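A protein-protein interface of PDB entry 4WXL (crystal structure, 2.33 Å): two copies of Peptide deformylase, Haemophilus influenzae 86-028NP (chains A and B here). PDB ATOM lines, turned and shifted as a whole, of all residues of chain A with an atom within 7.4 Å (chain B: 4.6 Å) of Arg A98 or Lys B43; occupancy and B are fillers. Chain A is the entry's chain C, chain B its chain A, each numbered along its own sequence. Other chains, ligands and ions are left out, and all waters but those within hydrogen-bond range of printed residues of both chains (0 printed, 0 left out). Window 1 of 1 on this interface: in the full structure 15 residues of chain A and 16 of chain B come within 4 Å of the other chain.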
ATOM      1  N   ILE A  87     -17.654  32.199  28.841  1.00  0.00           N
ATOM      2  CA  ILE A  87     -16.368  31.609  29.008  1.00  0.00           C
ATOM      3  C   ILE A  87     -15.852  31.370  27.603  1.00  0.00           C
ATOM      4  O   ILE A  87     -16.641  31.145  26.672  1.00  0.00           O
ATOM      5  CB  ILE A  87     -16.484  30.324  29.822  1.00  0.00           C
ATOM      6  CG1 ILE A  87     -15.181  30.101  30.599  1.00  0.00           C
ATOM      7  CG2 ILE A  87     -16.949  29.160  28.923  1.00  0.00           C
ATOM      8  CD1 ILE A  87     -14.695  28.665  30.645  1.00  0.00           C
ATOM      9  N   GLU A  88     -14.538  31.448  27.440  1.00  0.00           N
ATOM     10  CA  GLU A  88     -13.920  31.190  26.140  1.00  0.00           C
ATOM     11  C   GLU A  88     -14.234  29.769  25.809  1.00  0.00           C
ATOM     12  O   GLU A  88     -13.732  28.887  26.438  1.00  0.00           O
ATOM     13  CB  GLU A  88     -12.424  31.388  26.203  1.00  0.00           C
ATOM     14  CG  GLU A  88     -12.024  32.841  26.419  1.00  0.00           C
ATOM     15  CD  GLU A  88     -12.108  33.321  27.855  1.00  0.00           C
ATOM     16  OE1 GLU A  88     -12.429  32.557  28.782  1.00  0.00           O
ATOM     17  OE2 GLU A  88     -11.859  34.507  28.055  1.00  0.00           O
ATOM     18  N   GLU A  89     -15.167  29.562  24.897  1.00  0.00           N
ATOM     19  CA  GLU A  89     -15.658  28.221  24.557  1.00  0.00           C
ATOM     20  C   GLU A  89     -14.874  27.625  23.393  1.00  0.00           C
ATOM     21  O   GLU A  89     -14.528  28.362  22.432  1.00  0.00           O
ATOM     22  CB  GLU A  89     -17.075  28.314  24.056  1.00  0.00           C
ATOM     23  CG  GLU A  89     -18.077  28.528  25.123  1.00  0.00           C
ATOM     24  CD  GLU A  89     -19.459  28.665  24.549  1.00  0.00           C
ATOM     25  OE1 GLU A  89     -19.768  27.932  23.563  1.00  0.00           O
ATOM     26  OE2 GLU A  89     -20.236  29.462  25.109  1.00  0.00           O
ATOM     27  N   GLY A  90     -14.654  26.304  23.462  1.00  0.00           N
ATOM     28  CA  GLY A  90     -14.125  25.535  22.375  1.00  0.00           C
ATOM     29  C   GLY A  90     -15.131  24.503  21.851  1.00  0.00           C
ATOM     30  O   GLY A  90     -16.175  24.297  22.428  1.00  0.00           O
ATOM     31  N   CYS A  91     -14.766  23.852  20.756  1.00  0.00           N
ATOM     32  CA  CYS A  91     -15.616  22.952  19.982  1.00  0.00           C
ATOM     33  C   CYS A  91     -14.722  21.952  19.271  1.00  0.00           C
ATOM     34  O   CYS A  91     -13.701  22.318  18.620  1.00  0.00           O
ATOM     35  CB  CYS A  91     -16.355  23.740  18.937  1.00  0.00           C
ATOM     36  SG  CYS A  91     -17.714  22.924  18.104  1.00  0.00           S
ATOM     37  N   LEU A  92     -15.085  20.686  19.372  1.00  0.00           N
ATOM     38  CA  LEU A  92     -14.355  19.661  18.681  1.00  0.00           C
ATOM     39  C   LEU A  92     -14.472  19.840  17.192  1.00  0.00           C
ATOM     40  O   LEU A  92     -13.573  19.429  16.473  1.00  0.00           O
ATOM     41  CB  LEU A  92     -14.902  18.297  19.076  1.00  0.00           C
ATOM     42  CG  LEU A  92     -14.608  17.960  20.545  1.00  0.00           C
ATOM     43  CD1 LEU A  92     -15.452  16.772  20.980  1.00  0.00           C
ATOM     44  CD2 LEU A  92     -13.131  17.650  20.728  1.00  0.00           C
ATOM     45  N   ILE A  94     -14.273  22.664  15.797  1.00  0.00           N
ATOM     46  CA  ILE A  94     -13.470  23.864  15.468  1.00  0.00           C
ATOM     47  C   ILE A  94     -12.146  23.808  16.243  1.00  0.00           C
ATOM     48  O   ILE A  94     -11.873  24.650  17.126  1.00  0.00           O
ATOM     49  CB  ILE A  94     -14.242  25.164  15.750  1.00  0.00           C
ATOM     50  CG1 ILE A  94     -15.678  25.005  15.317  1.00  0.00           C
ATOM     51  CG2 ILE A  94     -13.623  26.307  14.990  1.00  0.00           C
ATOM     52  CD1 ILE A  94     -16.481  26.271  15.449  1.00  0.00           C
ATOM     53  N   PRO A  95     -11.339  22.777  15.950  1.00  0.00           N
ATOM     54  CA  PRO A  95     -10.271  22.420  16.846  1.00  0.00           C
ATOM     55  C   PRO A  95      -9.231  23.520  16.910  1.00  0.00           C
ATOM     56  O   PRO A  95      -8.981  24.167  15.911  1.00  0.00           O
ATOM     57  CB  PRO A  95      -9.705  21.144  16.224  1.00  0.00           C
ATOM     58  CG  PRO A  95     -10.080  21.222  14.794  1.00  0.00           C
ATOM     59  CD  PRO A  95     -11.438  21.837  14.827  1.00  0.00           C
ATOM     60  N   GLY A  96      -8.707  23.759  18.111  1.00  0.00           N
ATOM     61  CA  GLY A  96      -7.633  24.701  18.326  1.00  0.00           C
ATOM     62  C   GLY A  96      -8.076  26.138  18.523  1.00  0.00           C
ATOM     63  O   GLY A  96      -7.226  27.031  18.541  1.00  0.00           O
ATOM     64  N   PHE A  97      -9.377  26.389  18.690  1.00  0.00           N
ATOM     65  CA  PHE A  97      -9.839  27.758  18.871  1.00  0.00           C
ATOM     66  C   PHE A  97     -10.910  27.880  19.933  1.00  0.00           C
ATOM     67  O   PHE A  97     -11.715  26.979  20.108  1.00  0.00           O
ATOM     68  CB  PHE A  97     -10.400  28.286  17.576  1.00  0.00           C
ATOM     69  CG  PHE A  97      -9.397  28.392  16.485  1.00  0.00           C
ATOM     70  CD1 PHE A  97      -8.370  29.328  16.561  1.00  0.00           C
ATOM     71  CD2 PHE A  97      -9.469  27.563  15.376  1.00  0.00           C
ATOM     72  CE1 PHE A  97      -7.429  29.433  15.556  1.00  0.00           C
ATOM     73  CE2 PHE A  97      -8.536  27.664  14.376  1.00  0.00           C
ATOM     74  CZ  PHE A  97      -7.515  28.598  14.463  1.00  0.00           C
ATOM     75  N   ARG A  98     -10.887  28.983  20.672  1.00  0.00           N
ATOM     76  CA  ARG A  98     -11.996  29.308  21.575  1.00  0.00           C
ATOM     77  C   ARG A  98     -12.287  30.798  21.537  1.00  0.00           C
ATOM     78  O   ARG A  98     -11.453  31.589  21.122  1.00  0.00           O
ATOM     79  CB  ARG A  98     -11.797  28.752  23.000  1.00  0.00           C
ATOM     80  CG  ARG A  98     -10.450  28.107  23.207  1.00  0.00           C
ATOM     81  CD  ARG A  98     -10.423  26.776  23.937  1.00  0.00           C
ATOM     82  NE  ARG A  98      -9.470  25.828  23.315  1.00  0.00           N
ATOM     83  CZ  ARG A  98      -8.241  26.086  22.794  1.00  0.00           C
ATOM     84  NH1 ARG A  98      -7.651  27.291  22.807  1.00  0.00           N
ATOM     85  NH2 ARG A  98      -7.550  25.078  22.266  1.00  0.00           N
ATOM     86  N   ALA A  99     -13.507  31.149  21.920  1.00  0.00           N
ATOM     87  CA  ALA A  99     -13.979  32.536  21.938  1.00  0.00           C
ATOM     88  C   ALA A  99     -15.026  32.630  22.980  1.00  0.00           C
ATOM     89  O   ALA A  99     -15.819  31.681  23.157  1.00  0.00           O
ATOM     90  CB  ALA A  99     -14.610  32.934  20.607  1.00  0.00           C
ATOM     91  N   LEU A 100     -15.045  33.776  23.663  1.00  0.00           N
ATOM     92  CA  LEU A 100     -16.076  34.065  24.621  1.00  0.00           C
ATOM     93  C   LEU A 100     -17.382  34.235  23.879  1.00  0.00           C
ATOM     94  O   LEU A 100     -17.468  35.012  22.943  1.00  0.00           O
ATOM     95  CB  LEU A 100     -15.773  35.352  25.385  1.00  0.00           C
ATOM     96  CG  LEU A 100     -16.726  35.618  26.560  1.00  0.00           C
ATOM     97  CD1 LEU A 100     -15.962  36.323  27.655  1.00  0.00           C
ATOM     98  CD2 LEU A 100     -17.937  36.431  26.127  1.00  0.00           C
ATOM     99  N   VAL A 101     -18.405  33.511  24.304  1.00  0.00           N
ATOM    100  CA  VAL A 101     -19.698  33.648  23.691  1.00  0.00           C
ATOM    101  C   VAL A 101     -20.701  34.015  24.775  1.00  0.00           C
ATOM    102  O   VAL A 101     -20.754  33.370  25.843  1.00  0.00           O
ATOM    103  CB  VAL A 101     -20.075  32.361  22.919  1.00  0.00           C
ATOM    104  CG1 VAL A 101     -21.508  32.419  22.383  1.00  0.00           C
ATOM    105  CG2 VAL A 101     -19.103  32.167  21.769  1.00  0.00           C
ATOM    106  N   PHE A 143     -19.817  28.622  17.265  1.00  0.00           N
ATOM    107  CA  PHE A 143     -19.346  29.736  18.099  1.00  0.00           C
ATOM    108  C   PHE A 143     -18.708  30.836  17.244  1.00  0.00           C
ATOM    109  O   PHE A 143     -18.812  32.044  17.570  1.00  0.00           O
ATOM    110  CB  PHE A 143     -18.489  29.277  19.319  1.00  0.00           C
ATOM    111  CG  PHE A 143     -17.034  28.976  19.030  1.00  0.00           C
ATOM    112  CD1 PHE A 143     -16.140  29.976  18.672  1.00  0.00           C
ATOM    113  CD2 PHE A 143     -16.530  27.704  19.245  1.00  0.00           C
ATOM    114  CE1 PHE A 143     -14.791  29.680  18.455  1.00  0.00           C
ATOM    115  CE2 PHE A 143     -15.194  27.397  19.026  1.00  0.00           C
ATOM    116  CZ  PHE A 143     -14.321  28.385  18.628  1.00  0.00           C
ATOM    117  N   LEU A 147     -18.565  35.736  16.152  1.00  0.00           N
ATOM    118  CA  LEU A 147     -17.379  36.561  15.979  1.00  0.00           C
ATOM    119  C   LEU A 147     -17.594  37.473  14.803  1.00  0.00           C
ATOM    120  O   LEU A 147     -18.704  37.585  14.294  1.00  0.00           O
ATOM    121  CB  LEU A 147     -16.154  35.686  15.710  1.00  0.00           C
ATOM    122  CG  LEU A 147     -15.823  34.734  16.856  1.00  0.00           C
ATOM    123  CD1 LEU A 147     -14.733  33.735  16.494  1.00  0.00           C
ATOM    124  CD2 LEU A 147     -15.446  35.513  18.106  1.00  0.00           C
ATOM    125  N   LYS A 151     -12.512  37.526  12.006  1.00  0.00           N
ATOM    126  CA  LYS A 151     -12.049  36.469  12.873  1.00  0.00           C
ATOM    127  C   LYS A 151     -12.467  35.079  12.377  1.00  0.00           C
ATOM    128  O   LYS A 151     -11.675  34.132  12.405  1.00  0.00           O
ATOM    129  CB  LYS A 151     -12.545  36.689  14.299  1.00  0.00           C
ATOM    130  CG  LYS A 151     -11.619  37.526  15.168  1.00  0.00           C
ATOM    131  CD  LYS A 151     -11.429  36.852  16.526  1.00  0.00           C
ATOM    132  CE  LYS A 151     -10.727  37.741  17.544  1.00  0.00           C
ATOM    133  NZ  LYS A 151     -10.224  36.940  18.701  1.00  0.00           N
ATOM    134  N   ILE A 155     -10.375  31.879  10.879  1.00  0.00           N
ATOM    135  CA  ILE A 155     -10.464  30.542  11.439  1.00  0.00           C
ATOM    136  C   ILE A 155     -10.719  29.493  10.369  1.00  0.00           C
ATOM    137  O   ILE A 155     -10.060  28.440  10.370  1.00  0.00           O
ATOM    138  CB  ILE A 155     -11.531  30.453  12.540  1.00  0.00           C
ATOM    139  CG1 ILE A 155     -10.948  31.028  13.843  1.00  0.00           C
ATOM    140  CG2 ILE A 155     -11.949  29.005  12.749  1.00  0.00           C
ATOM    141  CD1 ILE A 155     -11.980  31.482  14.852  1.00  0.00           C
ATOM    142  N   LYS A 158      -7.402  28.673   8.484  1.00  0.00           N
ATOM    143  CA  LYS A 158      -6.562  27.717   9.205  1.00  0.00           C
ATOM    144  C   LYS A 158      -7.123  26.305   9.182  1.00  0.00           C
ATOM    145  O   LYS A 158      -6.377  25.307   9.140  1.00  0.00           O
ATOM    146  CB  LYS A 158      -6.329  28.140  10.662  1.00  0.00           C
ATOM    147  CG  LYS A 158      -5.235  29.198  10.828  1.00  0.00           C
ATOM    148  CD  LYS A 158      -4.334  28.964  12.049  1.00  0.00           C
ATOM    149  CE  LYS A 158      -3.377  27.774  11.896  1.00  0.00           C
ATOM    150  NZ  LYS A 158      -2.131  27.952  12.715  1.00  0.00           N
ATOM    151  N   LEU A 159      -8.440  26.210   9.229  1.00  0.00           N
ATOM    152  CA  LEU A 159      -9.056  24.909   9.381  1.00  0.00           C
ATOM    153  C   LEU A 159      -9.101  24.094   8.098  1.00  0.00           C
ATOM    154  O   LEU A 159      -8.933  22.864   8.139  1.00  0.00           O
ATOM    155  CB  LEU A 159     -10.426  25.031  10.082  1.00  0.00           C
ATOM    156  CG  LEU A 159     -10.282  25.247  11.602  1.00  0.00           C
ATOM    157  CD1 LEU A 159     -11.638  25.301  12.280  1.00  0.00           C
ATOM    158  CD2 LEU A 159      -9.430  24.173  12.263  1.00  0.00           C
ATOM    159  N   TYR A 162      -5.756  22.701   8.025  1.00  0.00           N
ATOM    160  CA  TYR A 162      -5.684  21.653   9.024  1.00  0.00           C
ATOM    161  C   TYR A 162      -6.338  20.367   8.511  1.00  0.00           C
ATOM    162  O   TYR A 162      -5.813  19.275   8.692  1.00  0.00           O
ATOM    163  CB  TYR A 162      -6.372  22.136  10.329  1.00  0.00           C
ATOM    164  CG  TYR A 162      -6.468  21.070  11.413  1.00  0.00           C
ATOM    165  CD1 TYR A 162      -5.368  20.765  12.220  1.00  0.00           C
ATOM    166  CD2 TYR A 162      -7.639  20.355  11.617  1.00  0.00           C
ATOM    167  CE1 TYR A 162      -5.437  19.786  13.194  1.00  0.00           C
ATOM    168  CE2 TYR A 162      -7.711  19.371  12.589  1.00  0.00           C
ATOM    169  CZ  TYR A 162      -6.607  19.097  13.373  1.00  0.00           C
ATOM    170  OH  TYR A 162      -6.663  18.143  14.346  1.00  0.00           O
ATOM    171  N   MET B  39       1.341  22.531  22.508  1.00  0.00           N
ATOM    172  CA  MET B  39       0.083  23.089  22.971  1.00  0.00           C
ATOM    173  C   MET B  39      -0.875  23.252  21.790  1.00  0.00           C
ATOM    174  O   MET B  39      -2.045  22.855  21.880  1.00  0.00           O
ATOM    175  CB  MET B  39       0.319  24.428  23.677  1.00  0.00           C
ATOM    176  CG  MET B  39      -0.765  24.847  24.664  1.00  0.00           C
ATOM    177  SD  MET B  39      -0.543  26.581  25.174  1.00  0.00           S
ATOM    178  CE  MET B  39      -0.515  27.406  23.590  1.00  0.00           C
ATOM    179  N   TYR B  40      -0.400  23.791  20.667  1.00  0.00           N
ATOM    180  CA  TYR B  40      -1.326  24.026  19.560  1.00  0.00           C
ATOM    181  C   TYR B  40      -1.754  22.698  18.937  1.00  0.00           C
ATOM    182  O   TYR B  40      -2.942  22.481  18.732  1.00  0.00           O
ATOM    183  CB  TYR B  40      -0.768  25.010  18.530  1.00  0.00           C
ATOM    184  CG  TYR B  40      -0.660  26.425  19.065  1.00  0.00           C
ATOM    185  CD1 TYR B  40      -1.671  26.989  19.834  1.00  0.00           C
ATOM    186  CD2 TYR B  40       0.472  27.205  18.808  1.00  0.00           C
ATOM    187  CE1 TYR B  40      -1.580  28.309  20.307  1.00  0.00           C
ATOM    188  CE2 TYR B  40       0.575  28.521  19.278  1.00  0.00           C
ATOM    189  CZ  TYR B  40      -0.442  29.051  20.049  1.00  0.00           C
ATOM    190  OH  TYR B  40      -0.303  30.307  20.528  1.00  0.00           O
ATOM    191  N   GLN B  41      -0.788  21.807  18.720  1.00  0.00           N
ATOM    192  CA  GLN B  41      -1.010  20.492  18.146  1.00  0.00           C
ATOM    193  C   GLN B  41      -2.002  19.734  18.958  1.00  0.00           C
ATOM    194  O   GLN B  41      -2.885  19.102  18.405  1.00  0.00           O
ATOM    195  CB  GLN B  41       0.284  19.713  18.157  1.00  0.00           C
ATOM    196  CG  GLN B  41       0.125  18.228  17.906  1.00  0.00           C
ATOM    197  CD  GLN B  41       0.476  17.866  16.484  1.00  0.00           C
ATOM    198  OE1 GLN B  41      -0.101  18.403  15.540  1.00  0.00           O
ATOM    199  NE2 GLN B  41       1.436  16.964  16.318  1.00  0.00           N
ATOM    200  N   GLU B  42      -1.853  19.799  20.283  1.00  0.00           N
ATOM    201  CA  GLU B  42      -2.724  19.075  21.201  1.00  0.00           C
ATOM    202  C   GLU B  42      -3.993  19.856  21.601  1.00  0.00           C
ATOM    203  O   GLU B  42      -4.782  19.373  22.409  1.00  0.00           O
ATOM    204  CB  GLU B  42      -1.943  18.703  22.440  1.00  0.00           C
ATOM    205  CG  GLU B  42      -0.819  17.696  22.192  1.00  0.00           C
ATOM    206  CD  GLU B  42      -1.326  16.268  22.054  1.00  0.00           C
ATOM    207  OE1 GLU B  42      -1.997  15.781  22.973  1.00  0.00           O
ATOM    208  OE2 GLU B  42      -1.091  15.629  21.025  1.00  0.00           O
ATOM    209  N   LYS B  43      -4.199  21.049  21.040  1.00  0.00           N
ATOM    210  CA  LYS B  43      -5.433  21.801  21.257  1.00  0.00           C
ATOM    211  C   LYS B  43      -5.601  22.158  22.746  1.00  0.00           C
ATOM    212  O   LYS B  43      -6.705  22.218  23.243  1.00  0.00           O
ATOM    213  CB  LYS B  43      -6.680  21.053  20.699  1.00  0.00           C
ATOM    214  CG  LYS B  43      -6.508  20.413  19.314  1.00  0.00           C
ATOM    215  CD  LYS B  43      -6.307  21.482  18.246  1.00  0.00           C
ATOM    216  CE  LYS B  43      -5.449  21.041  17.061  1.00  0.00           C
ATOM    217  NZ  LYS B  43      -5.278  22.117  16.023  1.00  0.00           N
ATOM    218  N   GLY B  44      -4.498  22.443  23.437  1.00  0.00           N
ATOM    219  CA  GLY B  44      -4.557  22.997  24.800  1.00  0.00           C
ATOM    220  C   GLY B  44      -4.520  24.519  24.823  1.00  0.00           C
ATOM    221  O   GLY B  44      -4.166  25.157  23.840  1.00  0.00           O
ATOM    222  N   ILE B  45      -4.899  25.098  25.936  1.00  0.00           N
ATOM    223  CA  ILE B  45      -4.814  26.539  26.081  1.00  0.00           C
ATOM    224  C   ILE B  45      -3.690  26.927  26.987  1.00  0.00           C
ATOM    225  O   ILE B  45      -3.325  28.090  27.015  1.00  0.00           O
ATOM    226  CB  ILE B  45      -6.085  27.177  26.658  1.00  0.00           C
ATOM    227  CG1 ILE B  45      -6.595  26.422  27.862  1.00  0.00           C
ATOM    228  CG2 ILE B  45      -7.137  27.225  25.593  1.00  0.00           C
ATOM    229  CD1 ILE B  45      -7.647  27.199  28.620  1.00  0.00           C
ATOM    230  N   ASP B  62      -2.300  30.469  25.840  1.00  0.00           N
ATOM    231  CA  ASP B  62      -2.994  31.138  24.715  1.00  0.00           C
ATOM    232  C   ASP B  62      -4.410  30.693  24.794  1.00  0.00           C
ATOM    233  O   ASP B  62      -4.744  29.620  24.304  1.00  0.00           O
ATOM    234  CB  ASP B  62      -2.455  30.703  23.344  1.00  0.00           C
ATOM    235  CG  ASP B  62      -3.089  31.454  22.203  1.00  0.00           C
ATOM    236  OD1 ASP B  62      -4.028  32.230  22.421  1.00  0.00           O
ATOM    237  OD2 ASP B  62      -2.628  31.287  21.076  1.00  0.00           O
ATOM    238  N   VAL B  63      -5.243  31.516  25.413  1.00  0.00           N
ATOM    239  CA  VAL B  63      -6.605  31.120  25.657  1.00  0.00           C
ATOM    240  C   VAL B  63      -7.359  31.027  24.334  1.00  0.00           C
ATOM    241  O   VAL B  63      -8.074  30.076  24.125  1.00  0.00           O
ATOM    242  CB  VAL B  63      -7.332  32.084  26.590  1.00  0.00           C
ATOM    243  CG1 VAL B  63      -8.802  31.731  26.671  1.00  0.00           C
ATOM    244  CG2 VAL B  63      -6.697  32.047  27.962  1.00  0.00           C
ATOM    245  N   GLU B  64      -7.211  31.994  23.434  1.00  0.00           N
ATOM    246  CA  GLU B  64      -8.026  31.938  22.212  1.00  0.00           C
ATOM    247  C   GLU B  64      -7.542  30.956  21.192  1.00  0.00           C
ATOM    248  O   GLU B  64      -8.341  30.353  20.444  1.00  0.00           O
ATOM    249  CB  GLU B  64      -8.172  33.299  21.568  1.00  0.00           C
ATOM    250  CG  GLU B  64      -9.604  33.777  21.682  1.00  0.00           C
ATOM    251  CD  GLU B  64      -9.690  35.133  22.287  1.00  0.00           C
ATOM    252  OE1 GLU B  64      -9.226  35.253  23.442  1.00  0.00           O
ATOM    253  OE2 GLU B  64     -10.201  36.041  21.595  1.00  0.00           O
ATOM    254  N   GLY B  65      -6.228  30.818  21.155  1.00  0.00           N
ATOM    255  CA  GLY B  65      -5.611  29.803  20.368  1.00  0.00           C
ATOM    256  C   GLY B  65      -5.232  30.339  19.016  1.00  0.00           C
ATOM    257  O   GLY B  65      -4.612  29.628  18.249  1.00  0.00           O
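O of Lys B43 lies within hydrogen-bond range of NH2 of Arg A98 (3.1 Å).
OE2 of Glu B64 is in salt-bridge range of NZ of Lys A151, at 3.0 Å.
The backbone NH (N) of Arg A98 is in hydrogen-bond range of the backbone carbonyl oxygen (O) of Glu B64 (2.9 Å).
The guanidinium group (NH1) of Arg A98 is in hydrogen-bond range of the backbone carbonyl oxygen (O) of Val B63 (3.1 Å).
CG1 of Val B63 touches CG of Glu A88, 3.4 Å away.
Lys B43 touches Pro A95.
CD of Lys B43 touches N of Gly A96 (3.3 Å).
Glu B64 touches Gly A96.
CA of Gly B65 touches O of Gly A96, 3.7 Å away.
Glu B64 touches Phe A97 (O to CA, 3.4 Å).
CE1 of Phe A97 touches O of Gly B65, at 3.9 Å.
NH2 of Arg A98 touches O of Gly B44 (3.7 Å).
Ile B45 touches Arg A98.
NZ of Lys B43 touches CE1 of Tyr A162 (3.7 Å).
No position is printed for both chains.
Of the 14 pairs that touch across the chains among the printed residues, none has its exchanged pair printed and touching as well.
Of the 21 printed residues of chain A, 7 touch a printed residue of chain B.
Printed residues of chain B that touch a printed residue of chain A: Lys B43, Gly B44, Ile B45, Val B63, Glu B64 and Gly B65.
OD1 of Asp B62 lies within hydrogen-bond range of N of Glu B64.
The backbone NH (N) of Gly B65 is in hydrogen-bond range of the side-chain carboxylate (OD1) of Asp B62 (2.9 Å).
The backbone NH (N) of Gly B44 lies within hydrogen-bond range of the backbone carbonyl oxygen (O) of Met B39, 2.9 Å away.
O of Ile B45 is in hydrogen-bond range of N of Asp B62, 2.8 Å away.
Of the printed residues of chain B, Arg A98 touches Lys B43, Gly B44, Ile B45, Val B63 and Glu B64.
Printed residues of chain A within 4 Å of Lys B43: Pro A95 (3.8 Å), Gly A96 (3.3 Å), Arg A98 (3.1 Å) and Tyr A162 (3.7 Å).
Of the printed residues of chain A, Val B63 touches Glu A88 (3.4 Å) and Arg A98 (3.1 Å).
Of the printed residues of chain B, Glu A88 touches Val B63 (3.4 Å).
Printed residues of chain A within 4 Å of Glu B64: Gly A96 (3.99 Å), Phe A97 (3.4 Å), Arg A98 (2.9 Å) and Lys A151 (3.0 Å).
Printed residues of chain A within 4 Å of Gly B65: Gly A96 (3.7 Å) and Phe A97 (3.9 Å).
Of the printed residues of chain A, Ile B45 touches Arg A98.
Ile A87 touches none of the printed residues of chain B.
The nearest printed residue of chain A that does not touch Glu B64 is Ala A99 (4.6 Å).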
